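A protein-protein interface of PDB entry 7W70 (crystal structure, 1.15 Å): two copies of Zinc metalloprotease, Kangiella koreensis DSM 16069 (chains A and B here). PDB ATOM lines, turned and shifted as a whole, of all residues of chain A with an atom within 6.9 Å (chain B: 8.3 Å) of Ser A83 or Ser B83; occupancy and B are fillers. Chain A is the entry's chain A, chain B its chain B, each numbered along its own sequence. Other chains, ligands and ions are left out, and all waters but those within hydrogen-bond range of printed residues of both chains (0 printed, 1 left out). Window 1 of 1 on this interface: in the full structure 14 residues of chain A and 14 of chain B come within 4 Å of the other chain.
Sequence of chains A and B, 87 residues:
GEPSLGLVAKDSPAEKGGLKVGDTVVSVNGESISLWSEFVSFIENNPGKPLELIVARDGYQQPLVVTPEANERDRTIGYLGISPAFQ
NE1 of Trp A36 is in hydrogen-bond range of OE1 of Gln B87 (2.7 Å).
The backbone NH of Gly A81 is in hydrogen-bond range of the chain-end carboxylate of Gln B87, at 2.8 Å.
The backbone NH of Gln B87 lies within hydrogen-bond range of the backbone carbonyl oxygen of Ile A82.
O of Pro A84 lies within hydrogen-bond range of OG of Ser B83, 3.1 Å away.
The backbone NH of Leu B80 is in hydrogen-bond range of the chain-end carboxylate of Gln A87.
OXT of Gln A87 lies within hydrogen-bond range of N of Gly B81, 2.7 Å away.
N of Ile B82 sits at hydrogen-bond distance from OXT of Gln A87 (2.9 Å).
No residue of chain B comes within 4 Å of Gly A6.
Of the printed residues of chain B, Leu A7 touches Phe B86 (3.4 Å).
Printed residues of chain B within 4 Å of Trp A36: Gln B87 (2.7 Å).
Of the printed residues of chain B, Ser A83 touches Leu B7 (3.5 Å), Ser B83 (3.5 Å), Pro B84 (3.99 Å) and Phe B86 (3.8 Å).
Pro A84 touches just these residues of chain B: Ser B83 (3.1 Å) and Pro B84 (3.6 Å).
Printed residues of chain B within 4 Å of Phe A86: Leu B7 (3.8 Å), Ala B9 (3.6 Å), Tyr B79 (3.5 Å), Gly B81 (3.6 Å), Ile B82 (3.4 Å) and Ser B83 (3.8 Å).
Of the printed residues of chain A, Tyr B79 touches Phe A86 (3.5 Å) and Gln A87 (3.3 Å).
Of the printed residues of chain A, Gln B87 touches Trp A36 (2.7 Å), Gly A81 (2.8 Å) and Ile A82 (2.8 Å).
The nearest printed residue of chain A that does not touch Ser B83 is Ala A85 (4.8 Å).
Among the printed residues, pairs that only touch across the chains: Leu A7 with Phe B86 (3.4 Å), Ala A9 with Phe B86 (3.7 Å), Gly A81 with Phe B86 (3.7 Å), Ile A82 with Phe B86 (3.3 Å), Ser A83 with Leu B7 (3.5 Å), Ser A83 with Ser B83 (3.5 Å), Ser A83 with Pro B84 (3.99 Å), Ser A83 with Phe B86 (3.8 Å), Pro A84 with Pro B84 (3.6 Å), Phe A86 with Leu B7 (3.8 Å), Phe A86 with Ala B9 (3.6 Å), Phe A86 with Tyr B79 (3.5 Å), Phe A86 with Gly B81 (3.6 Å), Phe A86 with Ile B82 (3.4 Å), Phe A86 with Ser B83 (3.8 Å), Gln A87 with Trp B36 (3.5 Å), Gln A87 with Val B40 (3.6 Å), Gln A87 with Ile B43 (3.7 Å) and Gln A87 with Tyr B79 (3.3 Å).
The backbone NH of Leu A7 sits at hydrogen-bond distance from the side-chain hydroxyl of Ser A83.
The backbone carbonyl oxygen (O) of Gly A81 is in hydrogen-bond range of the backbone NH (N) of Ala A9 (2.8 Å).
The backbone NH (N) of Gly B6 lies within hydrogen-bond range of the backbone carbonyl oxygen (O) of Ser B83 (3.0 Å).
The backbone NH (N) of Leu B7 sits at hydrogen-bond distance from the backbone carbonyl oxygen (O) of Ser B83 (2.9 Å).
N of Ala B9 sits at hydrogen-bond distance from O of Gly B81 (2.8 Å).
N of Ala B14 sits at hydrogen-bond distance from O of Leu B80 (2.9 Å).
Of the 14 printed residues of chain A, 9 touch a printed residue of chain B.
Hydrophobic or aromatic side chains of chain A that line the printed part of chain B: Leu A7, Trp A36, Ile A82, Pro A84 and Phe A86.
Along chain A the printed residues that touch a printed residue of chain B span positions 7 to 87.
Among the printed residues, 26 pairs touch across the chains.
Among the printed residues, no Asp or Glu carboxylate lies within 4 Å of a Lys or Arg side-chain nitrogen of the other chain.
Leu A7 touches Phe B86, and with the chains exchanged Phe A86 touches Leu B7.
Ala A9 touches Phe B86, and with the chains exchanged Phe A86 touches Ala B9.
Trp A36 touches Gln B87, and with the chains exchanged Gln A87 touches Trp B36.
Pro B84 touches its own counterpart, Pro A84.
Of the 26 pairs that touch across the chains among the printed residues, 20 have their exchanged pair printed and touching as well.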
ATOM      1  N   SER A   4      31.142 -22.210 -11.089  1.00  0.00           N
ATOM      2  CA  SER A   4      32.201 -22.896 -10.369  1.00  0.00           C
ATOM      3  C   SER A   4      31.631 -24.073  -9.593  1.00  0.00           C
ATOM      4  O   SER A   4      30.546 -23.986  -9.007  1.00  0.00           O
ATOM      5  CB  SER A   4      32.932 -21.944  -9.425  1.00  0.00           C
ATOM      6  OG  SER A   4      33.682 -20.998 -10.167  1.00  0.00           O
ATOM      7  N   LEU A   5      32.376 -25.172  -9.586  1.00  0.00           N
ATOM      8  CA  LEU A   5      31.907 -26.409  -8.992  1.00  0.00           C
ATOM      9  C   LEU A   5      32.163 -26.460  -7.504  1.00  0.00           C
ATOM     10  O   LEU A   5      33.252 -26.120  -7.036  1.00  0.00           O
ATOM     11  CB  LEU A   5      32.648 -27.599  -9.593  1.00  0.00           C
ATOM     12  CG  LEU A   5      32.130 -28.220 -10.882  1.00  0.00           C
ATOM     13  CD1 LEU A   5      32.171 -27.213 -12.002  1.00  0.00           C
ATOM     14  CD2 LEU A   5      32.960 -29.435 -11.236  1.00  0.00           C
ATOM     15  N   GLY A   6      31.161 -26.945  -6.779  1.00  0.00           N
ATOM     16  CA  GLY A   6      31.364 -27.461  -5.452  1.00  0.00           C
ATOM     17  C   GLY A   6      31.670 -28.939  -5.577  1.00  0.00           C
ATOM     18  O   GLY A   6      32.464 -29.342  -6.435  1.00  0.00           O
ATOM     19  N   LEU A   7      31.008 -29.758  -4.774  1.00  0.00           N
ATOM     20  CA  LEU A   7      31.378 -31.160  -4.650  1.00  0.00           C
ATOM     21  C   LEU A   7      31.058 -31.954  -5.917  1.00  0.00           C
ATOM     22  O   LEU A   7      30.124 -31.642  -6.666  1.00  0.00           O
ATOM     23  CB  LEU A   7      30.690 -31.775  -3.429  1.00  0.00           C
ATOM     24  CG  LEU A   7      30.988 -31.054  -2.110  1.00  0.00           C
ATOM     25  CD1 LEU A   7      30.290 -31.746  -0.953  1.00  0.00           C
ATOM     26  CD2 LEU A   7      32.489 -30.978  -1.868  1.00  0.00           C
ATOM     27  N   VAL A   8      31.858 -32.991  -6.145  1.00  0.00           N
ATOM     28  CA  VAL A   8      31.707 -33.903  -7.271  1.00  0.00           C
ATOM     29  C   VAL A   8      31.375 -35.276  -6.698  1.00  0.00           C
ATOM     30  O   VAL A   8      32.059 -35.750  -5.786  1.00  0.00           O
ATOM     31  CB  VAL A   8      32.995 -33.953  -8.114  1.00  0.00           C
ATOM     32  CG1 VAL A   8      32.886 -34.977  -9.238  1.00  0.00           C
ATOM     33  CG2 VAL A   8      33.311 -32.587  -8.690  1.00  0.00           C
ATOM     34  N   ALA A   9      30.324 -35.904  -7.214  1.00  0.00           N
ATOM     35  CA  ALA A   9      29.861 -37.171  -6.664  1.00  0.00           C
ATOM     36  C   ALA A   9      30.754 -38.331  -7.103  1.00  0.00           C
ATOM     37  O   ALA A   9      31.323 -38.335  -8.197  1.00  0.00           O
ATOM     38  CB  ALA A   9      28.413 -37.429  -7.081  1.00  0.00           C
ATOM     39  N   TRP A  36      25.831 -20.605 -13.927  1.00  0.00           N
ATOM     40  CA  TRP A  36      25.613 -22.001 -13.573  1.00  0.00           C
ATOM     41  C   TRP A  36      24.407 -22.582 -14.307  1.00  0.00           C
ATOM     42  O   TRP A  36      24.441 -23.734 -14.761  1.00  0.00           O
ATOM     43  CB  TRP A  36      25.424 -22.114 -12.057  1.00  0.00           C
ATOM     44  CG  TRP A  36      25.293 -23.515 -11.586  1.00  0.00           C
ATOM     45  CD1 TRP A  36      24.149 -24.140 -11.204  1.00  0.00           C
ATOM     46  CD2 TRP A  36      26.340 -24.478 -11.462  1.00  0.00           C
ATOM     47  NE1 TRP A  36      24.416 -25.439 -10.844  1.00  0.00           N
ATOM     48  CE2 TRP A  36      25.758 -25.668 -10.988  1.00  0.00           C
ATOM     49  CE3 TRP A  36      27.717 -24.448 -11.694  1.00  0.00           C
ATOM     50  CZ2 TRP A  36      26.500 -26.819 -10.759  1.00  0.00           C
ATOM     51  CZ3 TRP A  36      28.453 -25.589 -11.455  1.00  0.00           C
ATOM     52  CH2 TRP A  36      27.843 -26.756 -10.993  1.00  0.00           C
ATOM     53  N   GLY A  81      26.452 -35.263 -11.709  1.00  0.00           N
ATOM     54  CA  GLY A  81      26.984 -35.549 -10.388  1.00  0.00           C
ATOM     55  C   GLY A  81      27.787 -34.392  -9.826  1.00  0.00           C
ATOM     56  O   GLY A  81      28.851 -34.596  -9.229  1.00  0.00           O
ATOM     57  N   ILE A  82      27.296 -33.173 -10.013  1.00  0.00           N
ATOM     58  CA  ILE A  82      27.987 -31.984  -9.543  1.00  0.00           C
ATOM     59  C   ILE A  82      27.045 -31.091  -8.757  1.00  0.00           C
ATOM     60  O   ILE A  82      25.835 -31.043  -8.996  1.00  0.00           O
ATOM     61  CB  ILE A  82      28.616 -31.183 -10.694  1.00  0.00           C
ATOM     62  CG1 ILE A  82      27.513 -30.694 -11.628  1.00  0.00           C
ATOM     63  CG2 ILE A  82      29.690 -31.964 -11.398  1.00  0.00           C
ATOM     64  CD1 ILE A  82      28.019 -29.894 -12.731  1.00  0.00           C
ATOM     65  N   SER A  83      27.617 -30.385  -7.802  1.00  0.00           N
ATOM     66  CA  SER A  83      26.903 -29.342  -7.098  1.00  0.00           C
ATOM     67  C   SER A  83      27.609 -28.016  -7.332  1.00  0.00           C
ATOM     68  O   SER A  83      28.831 -27.988  -7.507  1.00  0.00           O
ATOM     69  CB  SER A  83      26.915 -29.637  -5.598  1.00  0.00           C
ATOM     70  OG  SER A  83      28.244 -29.609  -5.118  1.00  0.00           O
ATOM     71  N   PRO A  84      26.883 -26.907  -7.345  1.00  0.00           N
ATOM     72  CA  PRO A  84      27.543 -25.610  -7.488  1.00  0.00           C
ATOM     73  C   PRO A  84      28.325 -25.293  -6.224  1.00  0.00           C
ATOM     74  O   PRO A  84      28.103 -25.878  -5.162  1.00  0.00           O
ATOM     75  CB  PRO A  84      26.375 -24.638  -7.662  1.00  0.00           C
ATOM     76  CG  PRO A  84      25.252 -25.302  -6.951  1.00  0.00           C
ATOM     77  CD  PRO A  84      25.423 -26.770  -7.196  1.00  0.00           C
ATOM     78  N   ALA A  85      29.255 -24.355  -6.356  1.00  0.00           N
ATOM     79  CA  ALA A  85      30.048 -23.931  -5.209  1.00  0.00           C
ATOM     80  C   ALA A  85      29.136 -23.525  -4.058  1.00  0.00           C
ATOM     81  O   ALA A  85      28.076 -22.927  -4.269  1.00  0.00           O
ATOM     82  CB  ALA A  85      30.927 -22.749  -5.601  1.00  0.00           C
ATOM     83  N   PHE A  86      29.542 -23.882  -2.844  1.00  0.00           N
ATOM     84  CA  PHE A  86      28.760 -23.509  -1.670  1.00  0.00           C
ATOM     85  C   PHE A  86      28.567 -22.001  -1.625  1.00  0.00           C
ATOM     86  O   PHE A  86      29.482 -21.235  -1.937  1.00  0.00           O
ATOM     87  CB  PHE A  86      29.470 -23.957  -0.395  1.00  0.00           C
ATOM     88  CG  PHE A  86      29.377 -25.430  -0.130  1.00  0.00           C
ATOM     89  CD1 PHE A  86      28.183 -25.996   0.288  1.00  0.00           C
ATOM     90  CD2 PHE A  86      30.486 -26.243  -0.270  1.00  0.00           C
ATOM     91  CE1 PHE A  86      28.087 -27.356   0.541  1.00  0.00           C
ATOM     92  CE2 PHE A  86      30.403 -27.604  -0.014  1.00  0.00           C
ATOM     93  CZ  PHE A  86      29.198 -28.160   0.393  1.00  0.00           C
ATOM     94  N   GLN A  87      27.360 -21.580  -1.254  1.00  0.00           N
ATOM     95  CA  GLN A  87      27.071 -20.170  -1.072  1.00  0.00           C
ATOM     96  C   GLN A  87      26.707 -19.888   0.369  1.00  0.00           C
ATOM     97  O   GLN A  87      26.748 -18.721   0.775  1.00  0.00           O
ATOM     98  CB  GLN A  87      25.950 -19.733  -1.996  1.00  0.00           C
ATOM     99  CG  GLN A  87      26.297 -19.846  -3.465  1.00  0.00           C
ATOM    100  CD  GLN A  87      25.087 -19.685  -4.350  1.00  0.00           C
ATOM    101  OE1 GLN A  87      24.187 -20.526  -4.349  1.00  0.00           O
ATOM    102  NE2 GLN A  87      25.048 -18.593  -5.096  1.00  0.00           N
ATOM    103  OXT GLN A  87      26.385 -20.822   1.112  1.00  0.00           O
ATOM    104  N   GLU B   2      14.243 -24.817  -5.563  1.00  0.00           N
ATOM    105  CA  GLU B   2      13.630 -24.924  -4.242  1.00  0.00           C
ATOM    106  C   GLU B   2      14.662 -24.599  -3.160  1.00  0.00           C
ATOM    107  O   GLU B   2      15.821 -25.007  -3.272  1.00  0.00           O
ATOM    108  CB  GLU B   2      13.125 -26.358  -4.045  1.00  0.00           C
ATOM    109  CG  GLU B   2      12.361 -26.628  -2.752  1.00  0.00           C
ATOM    110  CD  GLU B   2      10.856 -26.549  -2.929  1.00  0.00           C
ATOM    111  OE1 GLU B   2      10.396 -26.362  -4.077  1.00  0.00           O
ATOM    112  OE2 GLU B   2      10.134 -26.674  -1.916  1.00  0.00           O
ATOM    113  N   PRO B   3      14.267 -23.852  -2.062  1.00  0.00           N
ATOM    114  CA  PRO B   3      15.196 -23.559  -0.963  1.00  0.00           C
ATOM    115  C   PRO B   3      15.384 -24.732   0.003  1.00  0.00           C
ATOM    116  O   PRO B   3      15.266 -24.574   1.234  1.00  0.00           O
ATOM    117  CB  PRO B   3      14.549 -22.346  -0.284  1.00  0.00           C
ATOM    118  CG  PRO B   3      13.141 -22.217  -0.897  1.00  0.00           C
ATOM    119  CD  PRO B   3      12.899 -23.463  -1.684  1.00  0.00           C
ATOM    120  N   SER B   4      15.684 -25.914  -0.568  1.00  0.00           N
ATOM    121  CA  SER B   4      15.858 -27.191   0.127  1.00  0.00           C
ATOM    122  C   SER B   4      17.313 -27.638   0.070  1.00  0.00           C
ATOM    123  O   SER B   4      17.859 -27.855  -1.018  1.00  0.00           O
ATOM    124  CB  SER B   4      15.018 -28.277  -0.543  1.00  0.00           C
ATOM    125  OG  SER B   4      14.803 -29.352   0.360  1.00  0.00           O
ATOM    126  N   LEU B   5      17.908 -27.867   1.235  1.00  0.00           N
ATOM    127  CA  LEU B   5      19.352 -28.015   1.328  1.00  0.00           C
ATOM    128  C   LEU B   5      19.778 -29.413   0.905  1.00  0.00           C
ATOM    129  O   LEU B   5      19.378 -30.410   1.512  1.00  0.00           O
ATOM    130  CB  LEU B   5      19.831 -27.724   2.745  1.00  0.00           C
ATOM    131  CG  LEU B   5      19.360 -26.404   3.344  1.00  0.00           C
ATOM    132  CD1 LEU B   5      20.015 -26.250   4.718  1.00  0.00           C
ATOM    133  CD2 LEU B   5      19.708 -25.248   2.429  1.00  0.00           C
ATOM    134  N   GLY B   6      20.619 -29.484  -0.119  1.00  0.00           N
ATOM    135  CA  GLY B   6      21.119 -30.767  -0.572  1.00  0.00           C
ATOM    136  C   GLY B   6      22.434 -31.082   0.101  1.00  0.00           C
ATOM    137  O   GLY B   6      22.746 -32.249   0.382  1.00  0.00           O
ATOM    138  N   LEU B   7      23.217 -30.038   0.362  1.00  0.00           N
ATOM    139  CA  LEU B   7      24.514 -30.185   0.991  1.00  0.00           C
ATOM    140  C   LEU B   7      24.737 -29.032   1.948  1.00  0.00           C
ATOM    141  O   LEU B   7      24.372 -27.889   1.651  1.00  0.00           O
ATOM    142  CB  LEU B   7      25.648 -30.182  -0.043  1.00  0.00           C
ATOM    143  CG  LEU B   7      25.569 -31.212  -1.171  1.00  0.00           C
ATOM    144  CD1 LEU B   7      26.442 -30.778  -2.311  1.00  0.00           C
ATOM    145  CD2 LEU B   7      25.973 -32.595  -0.686  1.00  0.00           C
ATOM    146  N   VAL B   8      25.345 -29.333   3.091  1.00  0.00           N
ATOM    147  CA  VAL B   8      25.698 -28.334   4.094  1.00  0.00           C
ATOM    148  C   VAL B   8      27.184 -28.491   4.382  1.00  0.00           C
ATOM    149  O   VAL B   8      27.619 -29.561   4.824  1.00  0.00           O
ATOM    150  CB  VAL B   8      24.876 -28.497   5.385  1.00  0.00           C
ATOM    151  CG1 VAL B   8      25.341 -27.502   6.457  1.00  0.00           C
ATOM    152  CG2 VAL B   8      23.391 -28.337   5.090  1.00  0.00           C
ATOM    153  N   ALA B   9      27.960 -27.434   4.138  1.00  0.00           N
ATOM    154  CA  ALA B   9      29.408 -27.514   4.285  1.00  0.00           C
ATOM    155  C   ALA B   9      29.811 -27.671   5.748  1.00  0.00           C
ATOM    156  O   ALA B   9      29.215 -27.072   6.648  1.00  0.00           O
ATOM    157  CB  ALA B   9      30.059 -26.264   3.698  1.00  0.00           C
ATOM    158  N   ALA B  14      26.157 -22.298   8.301  1.00  0.00           N
ATOM    159  CA  ALA B  14      24.946 -23.113   8.197  1.00  0.00           C
ATOM    160  C   ALA B  14      24.964 -24.264   9.199  1.00  0.00           C
ATOM    161  O   ALA B  14      23.992 -24.481   9.935  1.00  0.00           O
ATOM    162  CB  ALA B  14      24.780 -23.633   6.768  1.00  0.00           C
ATOM    163  N   VAL B  21      21.017 -31.200   5.999  1.00  0.00           N
ATOM    164  CA  VAL B  21      20.590 -31.675   4.694  1.00  0.00           C
ATOM    165  C   VAL B  21      19.130 -32.082   4.770  1.00  0.00           C
ATOM    166  O   VAL B  21      18.686 -32.721   5.732  1.00  0.00           O
ATOM    167  CB  VAL B  21      21.496 -32.835   4.243  1.00  0.00           C
ATOM    168  CG1 VAL B  21      20.868 -33.609   3.083  1.00  0.00           C
ATOM    169  CG2 VAL B  21      22.870 -32.307   3.873  1.00  0.00           C
ATOM    170  N   GLY B  22      18.366 -31.684   3.764  1.00  0.00           N
ATOM    171  CA  GLY B  22      16.958 -31.971   3.724  1.00  0.00           C
ATOM    172  C   GLY B  22      16.067 -30.881   4.279  1.00  0.00           C
ATOM    173  O   GLY B  22      14.855 -30.929   4.044  1.00  0.00           O
ATOM    174  N   ASP B  23      16.618 -29.907   5.010  1.00  0.00           N
ATOM    175  CA  ASP B  23      15.812 -28.808   5.516  1.00  0.00           C
ATOM    176  C   ASP B  23      15.304 -27.959   4.355  1.00  0.00           C
ATOM    177  O   ASP B  23      15.995 -27.747   3.348  1.00  0.00           O
ATOM    178  CB  ASP B  23      16.659 -27.909   6.417  1.00  0.00           C
ATOM    179  CG  ASP B  23      16.935 -28.508   7.785  1.00  0.00           C
ATOM    180  OD1 ASP B  23      16.397 -29.584   8.143  1.00  0.00           O
ATOM    181  OD2 ASP B  23      17.739 -27.868   8.508  1.00  0.00           O
ATOM    182  N   TRP B  36      15.216 -20.795  -3.934  1.00  0.00           N
ATOM    183  CA  TRP B  36      16.610 -20.867  -3.525  1.00  0.00           C
ATOM    184  C   TRP B  36      17.292 -19.511  -3.678  1.00  0.00           C
ATOM    185  O   TRP B  36      18.026 -19.064  -2.784  1.00  0.00           O
ATOM    186  CB  TRP B  36      17.330 -21.943  -4.357  1.00  0.00           C
ATOM    187  CG  TRP B  36      18.749 -22.134  -3.968  1.00  0.00           C
ATOM    188  CD1 TRP B  36      19.834 -21.463  -4.453  1.00  0.00           C
ATOM    189  CD2 TRP B  36      19.253 -23.062  -3.002  1.00  0.00           C
ATOM    190  NE1 TRP B  36      20.980 -21.911  -3.841  1.00  0.00           N
ATOM    191  CE2 TRP B  36      20.649 -22.891  -2.946  1.00  0.00           C
ATOM    192  CE3 TRP B  36      18.659 -24.020  -2.178  1.00  0.00           C
ATOM    193  CZ2 TRP B  36      21.459 -23.636  -2.094  1.00  0.00           C
ATOM    194  CZ3 TRP B  36      19.469 -24.768  -1.336  1.00  0.00           C
ATOM    195  CH2 TRP B  36      20.853 -24.569  -1.304  1.00  0.00           C
ATOM    196  N   PHE B  39      16.793 -17.100  -0.803  1.00  0.00           N
ATOM    197  CA  PHE B  39      17.638 -17.372   0.352  1.00  0.00           C
ATOM    198  C   PHE B  39      19.053 -16.887   0.098  1.00  0.00           C
ATOM    199  O   PHE B  39      19.659 -16.222   0.953  1.00  0.00           O
ATOM    200  CB  PHE B  39      17.612 -18.866   0.677  1.00  0.00           C
ATOM    201  CG  PHE B  39      18.217 -19.221   2.013  1.00  0.00           C
ATOM    202  CD1 PHE B  39      18.234 -18.326   3.074  1.00  0.00           C
ATOM    203  CD2 PHE B  39      18.757 -20.477   2.213  1.00  0.00           C
ATOM    204  CE1 PHE B  39      18.779 -18.689   4.307  1.00  0.00           C
ATOM    205  CE2 PHE B  39      19.307 -20.839   3.445  1.00  0.00           C
ATOM    206  CZ  PHE B  39      19.308 -19.947   4.485  1.00  0.00           C
ATOM    207  N   VAL B  40      19.578 -17.163  -1.098  1.00  0.00           N
ATOM    208  CA  VAL B  40      20.907 -16.687  -1.456  1.00  0.00           C
ATOM    209  C   VAL B  40      20.986 -15.166  -1.363  1.00  0.00           C
ATOM    210  O   VAL B  40      21.988 -14.618  -0.885  1.00  0.00           O
ATOM    211  CB  VAL B  40      21.303 -17.212  -2.847  1.00  0.00           C
ATOM    212  CG1 VAL B  40      22.601 -16.571  -3.300  1.00  0.00           C
ATOM    213  CG2 VAL B  40      21.427 -18.733  -2.833  1.00  0.00           C
ATOM    214  N   ILE B  43      21.436 -14.218   2.211  1.00  0.00           N
ATOM    215  CA  ILE B  43      22.759 -14.580   2.711  1.00  0.00           C
ATOM    216  C   ILE B  43      23.807 -13.613   2.191  1.00  0.00           C
ATOM    217  O   ILE B  43      24.595 -13.040   2.954  1.00  0.00           O
ATOM    218  CB  ILE B  43      23.094 -16.012   2.276  1.00  0.00           C
ATOM    219  CG1 ILE B  43      22.160 -17.019   2.959  1.00  0.00           C
ATOM    220  CG2 ILE B  43      24.569 -16.309   2.527  1.00  0.00           C
ATOM    221  CD1 ILE B  43      22.121 -18.382   2.247  1.00  0.00           C
ATOM    222  N   TYR B  79      28.353 -15.471   3.207  1.00  0.00           N
ATOM    223  CA  TYR B  79      28.501 -16.880   2.878  1.00  0.00           C
ATOM    224  C   TYR B  79      27.929 -17.710   4.017  1.00  0.00           C
ATOM    225  O   TYR B  79      28.218 -17.447   5.186  1.00  0.00           O
ATOM    226  CB  TYR B  79      29.986 -17.219   2.695  1.00  0.00           C
ATOM    227  CG  TYR B  79      30.285 -18.699   2.636  1.00  0.00           C
ATOM    228  CD1 TYR B  79      30.161 -19.397   1.444  1.00  0.00           C
ATOM    229  CD2 TYR B  79      30.708 -19.389   3.758  1.00  0.00           C
ATOM    230  CE1 TYR B  79      30.448 -20.748   1.371  1.00  0.00           C
ATOM    231  CE2 TYR B  79      30.991 -20.737   3.697  1.00  0.00           C
ATOM    232  CZ  TYR B  79      30.864 -21.411   2.503  1.00  0.00           C
ATOM    233  OH  TYR B  79      31.148 -22.762   2.460  1.00  0.00           O
ATOM    234  N   LEU B  80      27.145 -18.732   3.670  1.00  0.00           N
ATOM    235  CA  LEU B  80      26.529 -19.592   4.670  1.00  0.00           C
ATOM    236  C   LEU B  80      27.058 -21.013   4.663  1.00  0.00           C
ATOM    237  O   LEU B  80      27.237 -21.592   5.732  1.00  0.00           O
ATOM    238  CB  LEU B  80      25.014 -19.640   4.479  1.00  0.00           C
ATOM    239  CG  LEU B  80      24.276 -19.795   5.812  1.00  0.00           C
ATOM    240  CD1 LEU B  80      24.345 -18.486   6.630  1.00  0.00           C
ATOM    241  CD2 LEU B  80      22.827 -20.261   5.624  1.00  0.00           C
ATOM    242  N   GLY B  81      27.319 -21.591   3.488  1.00  0.00           N
ATOM    243  CA  GLY B  81      27.780 -22.968   3.371  1.00  0.00           C
ATOM    244  C   GLY B  81      26.717 -23.949   2.906  1.00  0.00           C
ATOM    245  O   GLY B  81      26.597 -25.048   3.464  1.00  0.00           O
ATOM    246  N   ILE B  82      25.925 -23.577   1.908  1.00  0.00           N
ATOM    247  CA  ILE B  82      24.835 -24.422   1.441  1.00  0.00           C
ATOM    248  C   ILE B  82      24.933 -24.608  -0.061  1.00  0.00           C
ATOM    249  O   ILE B  82      25.474 -23.767  -0.788  1.00  0.00           O
ATOM    250  CB  ILE B  82      23.447 -23.869   1.814  1.00  0.00           C
ATOM    251  CG1 ILE B  82      23.249 -22.481   1.198  1.00  0.00           C
ATOM    252  CG2 ILE B  82      23.298 -23.826   3.321  1.00  0.00           C
ATOM    253  CD1 ILE B  82      21.821 -21.969   1.265  1.00  0.00           C
ATOM    254  N   SER B  83      24.385 -25.730  -0.522  1.00  0.00           N
ATOM    255  CA  SER B  83      24.305 -25.993  -1.947  1.00  0.00           C
ATOM    256  C   SER B  83      23.108 -26.901  -2.175  1.00  0.00           C
ATOM    257  O   SER B  83      22.721 -27.651  -1.268  1.00  0.00           O
ATOM    258  CB  SER B  83      25.595 -26.656  -2.467  1.00  0.00           C
ATOM    259  OG  SER B  83      25.503 -27.005  -3.842  1.00  0.00           O
ATOM    260  N   PRO B  84      22.482 -26.829  -3.344  1.00  0.00           N
ATOM    261  CA  PRO B  84      21.451 -27.812  -3.692  1.00  0.00           C
ATOM    262  C   PRO B  84      22.068 -29.187  -3.920  1.00  0.00           C
ATOM    263  O   PRO B  84      23.288 -29.369  -3.965  1.00  0.00           O
ATOM    264  CB  PRO B  84      20.860 -27.267  -4.998  1.00  0.00           C
ATOM    265  CG  PRO B  84      21.350 -25.849  -5.098  1.00  0.00           C
ATOM    266  CD  PRO B  84      22.679 -25.847  -4.421  1.00  0.00           C
ATOM    267  N   ALA B  85      21.189 -30.173  -4.048  1.00  0.00           N
ATOM    268  CA  ALA B  85      21.626 -31.532  -4.318  1.00  0.00           C
ATOM    269  C   ALA B  85      22.348 -31.599  -5.666  1.00  0.00           C
ATOM    270  O   ALA B  85      22.262 -30.693  -6.500  1.00  0.00           O
ATOM    271  CB  ALA B  85      20.431 -32.485  -4.300  1.00  0.00           C
ATOM    272  N   PHE B  86      23.085 -32.691  -5.857  1.00  0.00           N
ATOM    273  CA  PHE B  86      23.813 -32.922  -7.101  1.00  0.00           C
ATOM    274  C   PHE B  86      22.874 -32.901  -8.305  1.00  0.00           C
ATOM    275  O   PHE B  86      21.723 -33.337  -8.237  1.00  0.00           O
ATOM    276  CB  PHE B  86      24.504 -34.287  -7.054  1.00  0.00           C
ATOM    277  CG  PHE B  86      25.615 -34.377  -6.049  1.00  0.00           C
ATOM    278  CD1 PHE B  86      26.810 -33.717  -6.257  1.00  0.00           C
ATOM    279  CD2 PHE B  86      25.478 -35.159  -4.914  1.00  0.00           C
ATOM    280  CE1 PHE B  86      27.845 -33.811  -5.344  1.00  0.00           C
ATOM    281  CE2 PHE B  86      26.510 -35.255  -3.991  1.00  0.00           C
ATOM    282  CZ  PHE B  86      27.694 -34.577  -4.209  1.00  0.00           C
ATOM    283  N   GLN B  87      23.383 -32.379  -9.417  1.00  0.00           N
ATOM    284  CA  GLN B  87      22.681 -32.448 -10.695  1.00  0.00           C
ATOM    285  C   GLN B  87      23.644 -32.864 -11.802  1.00  0.00           C
ATOM    286  O   GLN B  87      24.841 -33.020 -11.558  1.00  0.00           O
ATOM    287  CB  GLN B  87      22.019 -31.110 -11.011  1.00  0.00           C
ATOM    288  CG  GLN B  87      22.982 -29.946 -11.009  1.00  0.00           C
ATOM    289  CD  GLN B  87      22.292 -28.607 -10.751  1.00  0.00           C
ATOM    290  OE1 GLN B  87      22.929 -27.643 -10.324  1.00  0.00           O
ATOM    291  NE2 GLN B  87      20.985 -28.548 -11.005  1.00  0.00           N
ATOM    292  OXT GLN B  87      23.232 -33.072 -12.951  1.00  0.00           O
